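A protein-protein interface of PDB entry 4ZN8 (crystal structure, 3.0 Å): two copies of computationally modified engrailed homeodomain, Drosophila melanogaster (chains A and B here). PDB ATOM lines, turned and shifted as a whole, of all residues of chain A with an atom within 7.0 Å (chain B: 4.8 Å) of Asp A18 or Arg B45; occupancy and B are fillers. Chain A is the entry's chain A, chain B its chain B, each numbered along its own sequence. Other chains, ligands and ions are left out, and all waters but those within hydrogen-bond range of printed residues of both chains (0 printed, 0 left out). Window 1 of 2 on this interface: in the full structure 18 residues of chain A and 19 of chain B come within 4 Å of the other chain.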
ATOM      1  N   LEU A  13      -0.228 -13.277  -2.950  1.00  0.00           N
ATOM      2  CA  LEU A  13       0.145 -14.338  -2.024  1.00  0.00           C
ATOM      3  C   LEU A  13       1.145 -13.843  -0.987  1.00  0.00           C
ATOM      4  O   LEU A  13       0.960 -14.041   0.214  1.00  0.00           O
ATOM      5  CB  LEU A  13       0.730 -15.525  -2.796  1.00  0.00           C
ATOM      6  CG  LEU A  13       0.602 -16.943  -2.231  1.00  0.00           C
ATOM      7  CD1 LEU A  13       1.034 -17.948  -3.286  1.00  0.00           C
ATOM      8  CD2 LEU A  13       1.412 -17.135  -0.956  1.00  0.00           C
ATOM      9  N   LEU A  14       2.203 -13.194  -1.460  1.00  0.00           N
ATOM     10  CA  LEU A  14       3.288 -12.764  -0.588  1.00  0.00           C
ATOM     11  C   LEU A  14       2.894 -11.570   0.274  1.00  0.00           C
ATOM     12  O   LEU A  14       3.542 -11.286   1.280  1.00  0.00           O
ATOM     13  CB  LEU A  14       4.530 -12.433  -1.416  1.00  0.00           C
ATOM     14  CG  LEU A  14       5.010 -13.570  -2.321  1.00  0.00           C
ATOM     15  CD1 LEU A  14       6.303 -13.192  -3.027  1.00  0.00           C
ATOM     16  CD2 LEU A  14       5.182 -14.856  -1.528  1.00  0.00           C
ATOM     17  N   PHE A  15       1.831 -10.873  -0.118  1.00  0.00           N
ATOM     18  CA  PHE A  15       1.310  -9.776   0.689  1.00  0.00           C
ATOM     19  C   PHE A  15       0.587 -10.326   1.913  1.00  0.00           C
ATOM     20  O   PHE A  15       0.745  -9.815   3.021  1.00  0.00           O
ATOM     21  CB  PHE A  15       0.372  -8.888  -0.131  1.00  0.00           C
ATOM     22  CG  PHE A  15      -0.216  -7.743   0.648  1.00  0.00           C
ATOM     23  CD1 PHE A  15       0.518  -6.591   0.875  1.00  0.00           C
ATOM     24  CD2 PHE A  15      -1.506  -7.819   1.151  1.00  0.00           C
ATOM     25  CE1 PHE A  15      -0.020  -5.537   1.591  1.00  0.00           C
ATOM     26  CE2 PHE A  15      -2.049  -6.769   1.868  1.00  0.00           C
ATOM     27  CZ  PHE A  15      -1.305  -5.627   2.088  1.00  0.00           C
ATOM     28  N   LEU A  16      -0.208 -11.370   1.701  1.00  0.00           N
ATOM     29  CA  LEU A  16      -0.922 -12.030   2.787  1.00  0.00           C
ATOM     30  C   LEU A  16       0.052 -12.766   3.697  1.00  0.00           C
ATOM     31  O   LEU A  16      -0.117 -12.793   4.916  1.00  0.00           O
ATOM     32  CB  LEU A  16      -1.964 -13.002   2.230  1.00  0.00           C
ATOM     33  CG  LEU A  16      -3.047 -12.384   1.346  1.00  0.00           C
ATOM     34  CD1 LEU A  16      -3.908 -13.468   0.719  1.00  0.00           C
ATOM     35  CD2 LEU A  16      -3.901 -11.415   2.148  1.00  0.00           C
ATOM     36  N   PHE A  17       1.072 -13.363   3.087  1.00  0.00           N
ATOM     37  CA  PHE A  17       2.110 -14.065   3.828  1.00  0.00           C
ATOM     38  C   PHE A  17       2.885 -13.090   4.708  1.00  0.00           C
ATOM     39  O   PHE A  17       3.078 -13.336   5.897  1.00  0.00           O
ATOM     40  CB  PHE A  17       3.052 -14.791   2.864  1.00  0.00           C
ATOM     41  CG  PHE A  17       4.121 -15.596   3.546  1.00  0.00           C
ATOM     42  CD1 PHE A  17       3.788 -16.594   4.449  1.00  0.00           C
ATOM     43  CD2 PHE A  17       5.460 -15.371   3.268  1.00  0.00           C
ATOM     44  CE1 PHE A  17       4.770 -17.339   5.073  1.00  0.00           C
ATOM     45  CE2 PHE A  17       6.446 -16.115   3.888  1.00  0.00           C
ATOM     46  CZ  PHE A  17       6.101 -17.100   4.790  1.00  0.00           C
ATOM     47  N   ASP A  18       3.314 -11.977   4.119  1.00  0.00           N
ATOM     48  CA  ASP A  18       4.051 -10.952   4.851  1.00  0.00           C
ATOM     49  C   ASP A  18       3.193 -10.303   5.932  1.00  0.00           C
ATOM     50  O   ASP A  18       3.685  -9.985   7.015  1.00  0.00           O
ATOM     51  CB  ASP A  18       4.575  -9.882   3.893  1.00  0.00           C
ATOM     52  CG  ASP A  18       5.227  -8.721   4.615  1.00  0.00           C
ATOM     53  OD1 ASP A  18       5.987  -8.965   5.576  1.00  0.00           O
ATOM     54  OD2 ASP A  18       4.976  -7.562   4.224  1.00  0.00           O
ATOM     55  N   ARG A  19       1.914 -10.106   5.633  1.00  0.00           N
ATOM     56  CA  ARG A  19       1.002  -9.490   6.587  1.00  0.00           C
ATOM     57  C   ARG A  19       0.795 -10.409   7.783  1.00  0.00           C
ATOM     58  O   ARG A  19       0.686  -9.951   8.917  1.00  0.00           O
ATOM     59  CB  ARG A  19      -0.343  -9.167   5.933  1.00  0.00           C
ATOM     60  CG  ARG A  19      -1.005  -7.911   6.474  1.00  0.00           C
ATOM     61  CD  ARG A  19      -2.508  -7.927   6.255  1.00  0.00           C
ATOM     62  NE  ARG A  19      -3.205  -8.583   7.358  1.00  0.00           N
ATOM     63  CZ  ARG A  19      -4.525  -8.726   7.430  1.00  0.00           C
ATOM     64  NH1 ARG A  19      -5.298  -8.263   6.458  1.00  0.00           N
ATOM     65  NH2 ARG A  19      -5.071  -9.335   8.475  1.00  0.00           N
ATOM     66  N   ARG A  20       0.749 -11.710   7.515  1.00  0.00           N
ATOM     67  CA  ARG A  20       0.557 -12.708   8.560  1.00  0.00           C
ATOM     68  C   ARG A  20       1.810 -12.863   9.419  1.00  0.00           C
ATOM     69  O   ARG A  20       1.722 -12.985  10.640  1.00  0.00           O
ATOM     70  CB  ARG A  20       0.168 -14.052   7.942  1.00  0.00           C
ATOM     71  CG  ARG A  20       0.052 -15.188   8.939  1.00  0.00           C
ATOM     72  CD  ARG A  20      -1.032 -14.928   9.971  1.00  0.00           C
ATOM     73  NE  ARG A  20      -1.072 -15.988  10.971  1.00  0.00           N
ATOM     74  CZ  ARG A  20      -1.756 -17.119  10.834  1.00  0.00           C
ATOM     75  NH1 ARG A  20      -2.469 -17.338   9.738  1.00  0.00           N
ATOM     76  NH2 ARG A  20      -1.730 -18.029  11.797  1.00  0.00           N
ATOM     77  N   MET A  21       2.974 -12.851   8.776  1.00  0.00           N
ATOM     78  CA  MET A  21       4.240 -12.964   9.493  1.00  0.00           C
ATOM     79  C   MET A  21       4.488 -11.731  10.357  1.00  0.00           C
ATOM     80  O   MET A  21       5.127 -11.816  11.404  1.00  0.00           O
ATOM     81  CB  MET A  21       5.403 -13.163   8.518  1.00  0.00           C
ATOM     82  CG  MET A  21       5.349 -14.456   7.716  1.00  0.00           C
ATOM     83  SD  MET A  21       5.296 -16.071   8.810  1.00  0.00           S
ATOM     84  CE  MET A  21       3.401 -16.494   8.649  1.00  0.00           C
ATOM     85  N   THR A  22       3.981 -10.587   9.909  1.00  0.00           N
ATOM     86  CA  THR A  22       4.129  -9.341  10.650  1.00  0.00           C
ATOM     87  C   THR A  22       3.279  -9.371  11.916  1.00  0.00           C
ATOM     88  O   THR A  22       3.687  -8.863  12.962  1.00  0.00           O
ATOM     89  CB  THR A  22       3.738  -8.122   9.794  1.00  0.00           C
ATOM     90  OG1 THR A  22       4.431  -8.175   8.540  1.00  0.00           O
ATOM     91  CG2 THR A  22       4.096  -6.827  10.510  1.00  0.00           C
ATOM     92  N   GLU A  23       2.096  -9.971  11.813  1.00  0.00           N
ATOM     93  CA  GLU A  23       1.237 -10.175  12.974  1.00  0.00           C
ATOM     94  C   GLU A  23       1.941 -11.045  14.005  1.00  0.00           C
ATOM     95  O   GLU A  23       2.059 -10.676  15.174  1.00  0.00           O
ATOM     96  CB  GLU A  23      -0.086 -10.830  12.571  1.00  0.00           C
ATOM     97  CG  GLU A  23      -0.939 -10.029  11.610  1.00  0.00           C
ATOM     98  CD  GLU A  23      -2.117 -10.829  11.086  1.00  0.00           C
ATOM     99  OE1 GLU A  23      -2.412 -11.899  11.661  1.00  0.00           O
ATOM    100  OE2 GLU A  23      -2.744 -10.395  10.097  1.00  0.00           O
ATOM    101  N   ASP B  18      13.892  -6.684   8.664  1.00  0.00           N
ATOM    102  CA  ASP B  18      12.695  -6.598   7.833  1.00  0.00           C
ATOM    103  C   ASP B  18      12.956  -5.632   6.685  1.00  0.00           C
ATOM    104  O   ASP B  18      12.359  -5.738   5.612  1.00  0.00           O
ATOM    105  CB  ASP B  18      11.486  -6.148   8.654  1.00  0.00           C
ATOM    106  CG  ASP B  18      10.212  -6.085   7.830  1.00  0.00           C
ATOM    107  OD1 ASP B  18       9.500  -7.109   7.752  1.00  0.00           O
ATOM    108  OD2 ASP B  18       9.919  -5.011   7.264  1.00  0.00           O
ATOM    109  N   ARG B  25      13.409  -9.215  -1.492  1.00  0.00           N
ATOM    110  CA  ARG B  25      12.188  -9.781  -2.050  1.00  0.00           C
ATOM    111  C   ARG B  25      11.838  -9.077  -3.353  1.00  0.00           C
ATOM    112  O   ARG B  25      11.508  -9.717  -4.350  1.00  0.00           O
ATOM    113  CB  ARG B  25      11.027  -9.662  -1.061  1.00  0.00           C
ATOM    114  CG  ARG B  25       9.702 -10.162  -1.616  1.00  0.00           C
ATOM    115  CD  ARG B  25       8.560  -9.914  -0.646  1.00  0.00           C
ATOM    116  NE  ARG B  25       8.351  -8.490  -0.402  1.00  0.00           N
ATOM    117  CZ  ARG B  25       7.394  -8.001   0.380  1.00  0.00           C
ATOM    118  NH1 ARG B  25       6.553  -8.823   0.993  1.00  0.00           N
ATOM    119  NH2 ARG B  25       7.276  -6.692   0.547  1.00  0.00           N
ATOM    120  N   ARG B  42       5.998  -0.282  -5.214  1.00  0.00           N
ATOM    121  CA  ARG B  42       4.834   0.547  -4.953  1.00  0.00           C
ATOM    122  C   ARG B  42       3.531  -0.114  -5.411  1.00  0.00           C
ATOM    123  O   ARG B  42       2.462   0.482  -5.323  1.00  0.00           O
ATOM    124  CB  ARG B  42       5.021   1.916  -5.609  1.00  0.00           C
ATOM    125  CG  ARG B  42       4.131   2.991  -5.033  1.00  0.00           C
ATOM    126  CD  ARG B  42       4.811   3.785  -3.925  1.00  0.00           C
ATOM    127  NE  ARG B  42       3.818   4.383  -3.033  1.00  0.00           N
ATOM    128  CZ  ARG B  42       3.387   3.827  -1.903  1.00  0.00           C
ATOM    129  NH1 ARG B  42       3.880   2.665  -1.495  1.00  0.00           N
ATOM    130  NH2 ARG B  42       2.472   4.443  -1.167  1.00  0.00           N
ATOM    131  N   TRP B  43       3.607  -1.351  -5.889  1.00  0.00           N
ATOM    132  CA  TRP B  43       2.392  -2.150  -5.949  1.00  0.00           C
ATOM    133  C   TRP B  43       2.158  -2.618  -4.523  1.00  0.00           C
ATOM    134  O   TRP B  43       1.050  -2.527  -3.993  1.00  0.00           O
ATOM    135  CB  TRP B  43       2.503  -3.331  -6.913  1.00  0.00           C
ATOM    136  CG  TRP B  43       1.248  -4.161  -6.949  1.00  0.00           C
ATOM    137  CD1 TRP B  43       0.213  -4.055  -7.835  1.00  0.00           C
ATOM    138  CD2 TRP B  43       0.888  -5.210  -6.041  1.00  0.00           C
ATOM    139  NE1 TRP B  43      -0.762  -4.977  -7.539  1.00  0.00           N
ATOM    140  CE2 TRP B  43      -0.371  -5.698  -6.440  1.00  0.00           C
ATOM    141  CE3 TRP B  43       1.513  -5.786  -4.930  1.00  0.00           C
ATOM    142  CZ2 TRP B  43      -1.016  -6.735  -5.770  1.00  0.00           C
ATOM    143  CZ3 TRP B  43       0.871  -6.811  -4.265  1.00  0.00           C
ATOM    144  CH2 TRP B  43      -0.379  -7.276  -4.687  1.00  0.00           C
ATOM    145  N   PHE B  44       3.230  -3.114  -3.912  1.00  0.00           N
ATOM    146  CA  PHE B  44       3.250  -3.406  -2.487  1.00  0.00           C
ATOM    147  C   PHE B  44       3.070  -2.124  -1.694  1.00  0.00           C
ATOM    148  O   PHE B  44       3.501  -1.055  -2.129  1.00  0.00           O
ATOM    149  CB  PHE B  44       4.560  -4.078  -2.080  1.00  0.00           C
ATOM    150  CG  PHE B  44       4.635  -5.530  -2.429  1.00  0.00           C
ATOM    151  CD1 PHE B  44       4.076  -6.485  -1.596  1.00  0.00           C
ATOM    152  CD2 PHE B  44       5.278  -5.945  -3.580  1.00  0.00           C
ATOM    153  CE1 PHE B  44       4.150  -7.825  -1.912  1.00  0.00           C
ATOM    154  CE2 PHE B  44       5.355  -7.282  -3.901  1.00  0.00           C
ATOM    155  CZ  PHE B  44       4.790  -8.225  -3.067  1.00  0.00           C
ATOM    156  N   ARG B  45       2.422  -2.237  -0.540  1.00  0.00           N
ATOM    157  CA  ARG B  45       2.226  -1.117   0.380  1.00  0.00           C
ATOM    158  C   ARG B  45       1.461   0.056  -0.247  1.00  0.00           C
ATOM    159  O   ARG B  45       1.271   1.092   0.390  1.00  0.00           O
ATOM    160  CB  ARG B  45       3.576  -0.648   0.930  1.00  0.00           C
ATOM    161  CG  ARG B  45       4.306  -1.729   1.718  1.00  0.00           C
ATOM    162  CD  ARG B  45       3.533  -2.117   2.974  1.00  0.00           C
ATOM    163  NE  ARG B  45       4.198  -3.167   3.742  1.00  0.00           N
ATOM    164  CZ  ARG B  45       3.650  -3.799   4.776  1.00  0.00           C
ATOM    165  NH1 ARG B  45       2.426  -3.482   5.174  1.00  0.00           N
ATOM    166  NH2 ARG B  45       4.324  -4.743   5.418  1.00  0.00           N
ATOM    167  N   ARG B  46       1.037  -0.108  -1.496  1.00  0.00           N
ATOM    168  CA  ARG B  46      -0.053   0.687  -2.040  1.00  0.00           C
ATOM    169  C   ARG B  46      -1.276  -0.222  -2.022  1.00  0.00           C
ATOM    170  O   ARG B  46      -2.324   0.098  -2.582  1.00  0.00           O
ATOM    171  CB  ARG B  46       0.244   1.193  -3.455  1.00  0.00           C
ATOM    172  CG  ARG B  46       0.300   2.722  -3.583  1.00  0.00           C
ATOM    173  CD  ARG B  46      -0.011   3.194  -5.016  1.00  0.00           C
ATOM    174  NE  ARG B  46      -0.109   4.651  -5.140  1.00  0.00           N
ATOM    175  CZ  ARG B  46       0.854   5.458  -5.579  1.00  0.00           C
ATOM    176  NH1 ARG B  46       2.010   4.965  -6.005  1.00  0.00           N
ATOM    177  NH2 ARG B  46       0.634   6.766  -5.629  1.00  0.00           N
ATOM    178  N   LYS B  47      -1.110  -1.383  -1.396  1.00  0.00           N
ATOM    179  CA  LYS B  47      -2.218  -2.299  -1.158  1.00  0.00           C
ATOM    180  C   LYS B  47      -2.664  -2.158   0.292  1.00  0.00           C
ATOM    181  O   LYS B  47      -3.615  -2.805   0.735  1.00  0.00           O
ATOM    182  CB  LYS B  47      -1.822  -3.743  -1.473  1.00  0.00           C
ATOM    183  CG  LYS B  47      -3.018  -4.670  -1.623  1.00  0.00           C
ATOM    184  CD  LYS B  47      -2.666  -5.977  -2.302  1.00  0.00           C
ATOM    185  CE  LYS B  47      -3.921  -6.803  -2.533  1.00  0.00           C
ATOM    186  NZ  LYS B  47      -3.627  -8.117  -3.160  1.00  0.00           N
ATOM    187  N   GLU B  48      -1.958  -1.310   1.033  1.00  0.00           N
ATOM    188  CA  GLU B  48      -2.454  -0.842   2.318  1.00  0.00           C
ATOM    189  C   GLU B  48      -3.330   0.374   2.069  1.00  0.00           C
ATOM    190  O   GLU B  48      -4.113   0.779   2.928  1.00  0.00           O
ATOM    191  CB  GLU B  48      -1.313  -0.508   3.275  1.00  0.00           C
ATOM    192  CG  GLU B  48      -0.363  -1.662   3.511  1.00  0.00           C
ATOM    193  CD  GLU B  48      -0.272  -2.036   4.976  1.00  0.00           C
ATOM    194  OE1 GLU B  48      -0.547  -1.169   5.833  1.00  0.00           O
ATOM    195  OE2 GLU B  48       0.064  -3.202   5.270  1.00  0.00           O
ATOM    196  N   GLN B  49      -3.187   0.948   0.878  1.00  0.00           N
ATOM    197  CA  GLN B  49      -4.175   1.886   0.367  1.00  0.00           C
ATOM    198  C   GLN B  49      -5.511   1.155   0.269  1.00  0.00           C
ATOM    199  O   GLN B  49      -6.568   1.710   0.569  1.00  0.00           O
ATOM    200  CB  GLN B  49      -3.764   2.433  -1.002  1.00  0.00           C
ATOM    201  CG  GLN B  49      -3.755   3.952  -1.110  1.00  0.00           C
ATOM    202  CD  GLN B  49      -2.518   4.584  -0.505  1.00  0.00           C
ATOM    203  OE1 GLN B  49      -1.401   4.108  -0.705  1.00  0.00           O
ATOM    204  NE2 GLN B  49      -2.710   5.674   0.226  1.00  0.00           N
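The side-chain carboxylate (OD2) of Asp A18 is in salt-bridge range of the guanidinium group (NH1) of Arg B25 (3.8 Å). OD2 of Asp A18 is in salt-bridge range of NH2 of Arg B45 (3.1 Å).
The side-chain hydroxyl (OG1) of Thr A22 sits at hydrogen-bond distance from the backbone carbonyl oxygen (O) of Asp A18 (2.5 Å). NH1 of Arg B45 lies within salt-bridge range of OE1 of Glu B48 (3.8 Å).
Among the printed residues, pairs that only touch across the chains: Phe A15 with Lys B47 (3.9 Å) and Leu A14 with Arg B25 (3.9 Å).
Of chain B, only Arg B25 and Arg B45 come within 4 Å of Asp A18. Arg B45 touches just one residue of chain A: Asp A18 (3.1 Å). Of the printed residues of chain B, Leu A14 touches Arg B25. Of the printed residues of chain A, Lys B47 touches Phe A15 (3.9 Å). Of the printed residues of chain A, Arg B25 touches Leu A14 (3.9 Å) and Asp A18 (3.7 Å). Printed residues of chain B within 4 Å of Phe A15: Lys B47. The nearest residue of chain B that does not touch Asp A18 is Asp B18 (4.5 Å). The nearest printed residue of chain B that does not touch Phe A15 is Glu B48 (4.2 Å).
Printed residues of chain A that touch a printed residue of chain B: Leu A14, Phe A15 and Asp A18. Hydrophobic or aromatic side chains of chain A within 4 Å of the printed part of chain B: Phe A15.
1 position is printed for both chains. Of the 4 pairs that touch across the chains among the printed residues, none has its exchanged pair printed and touching as well.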
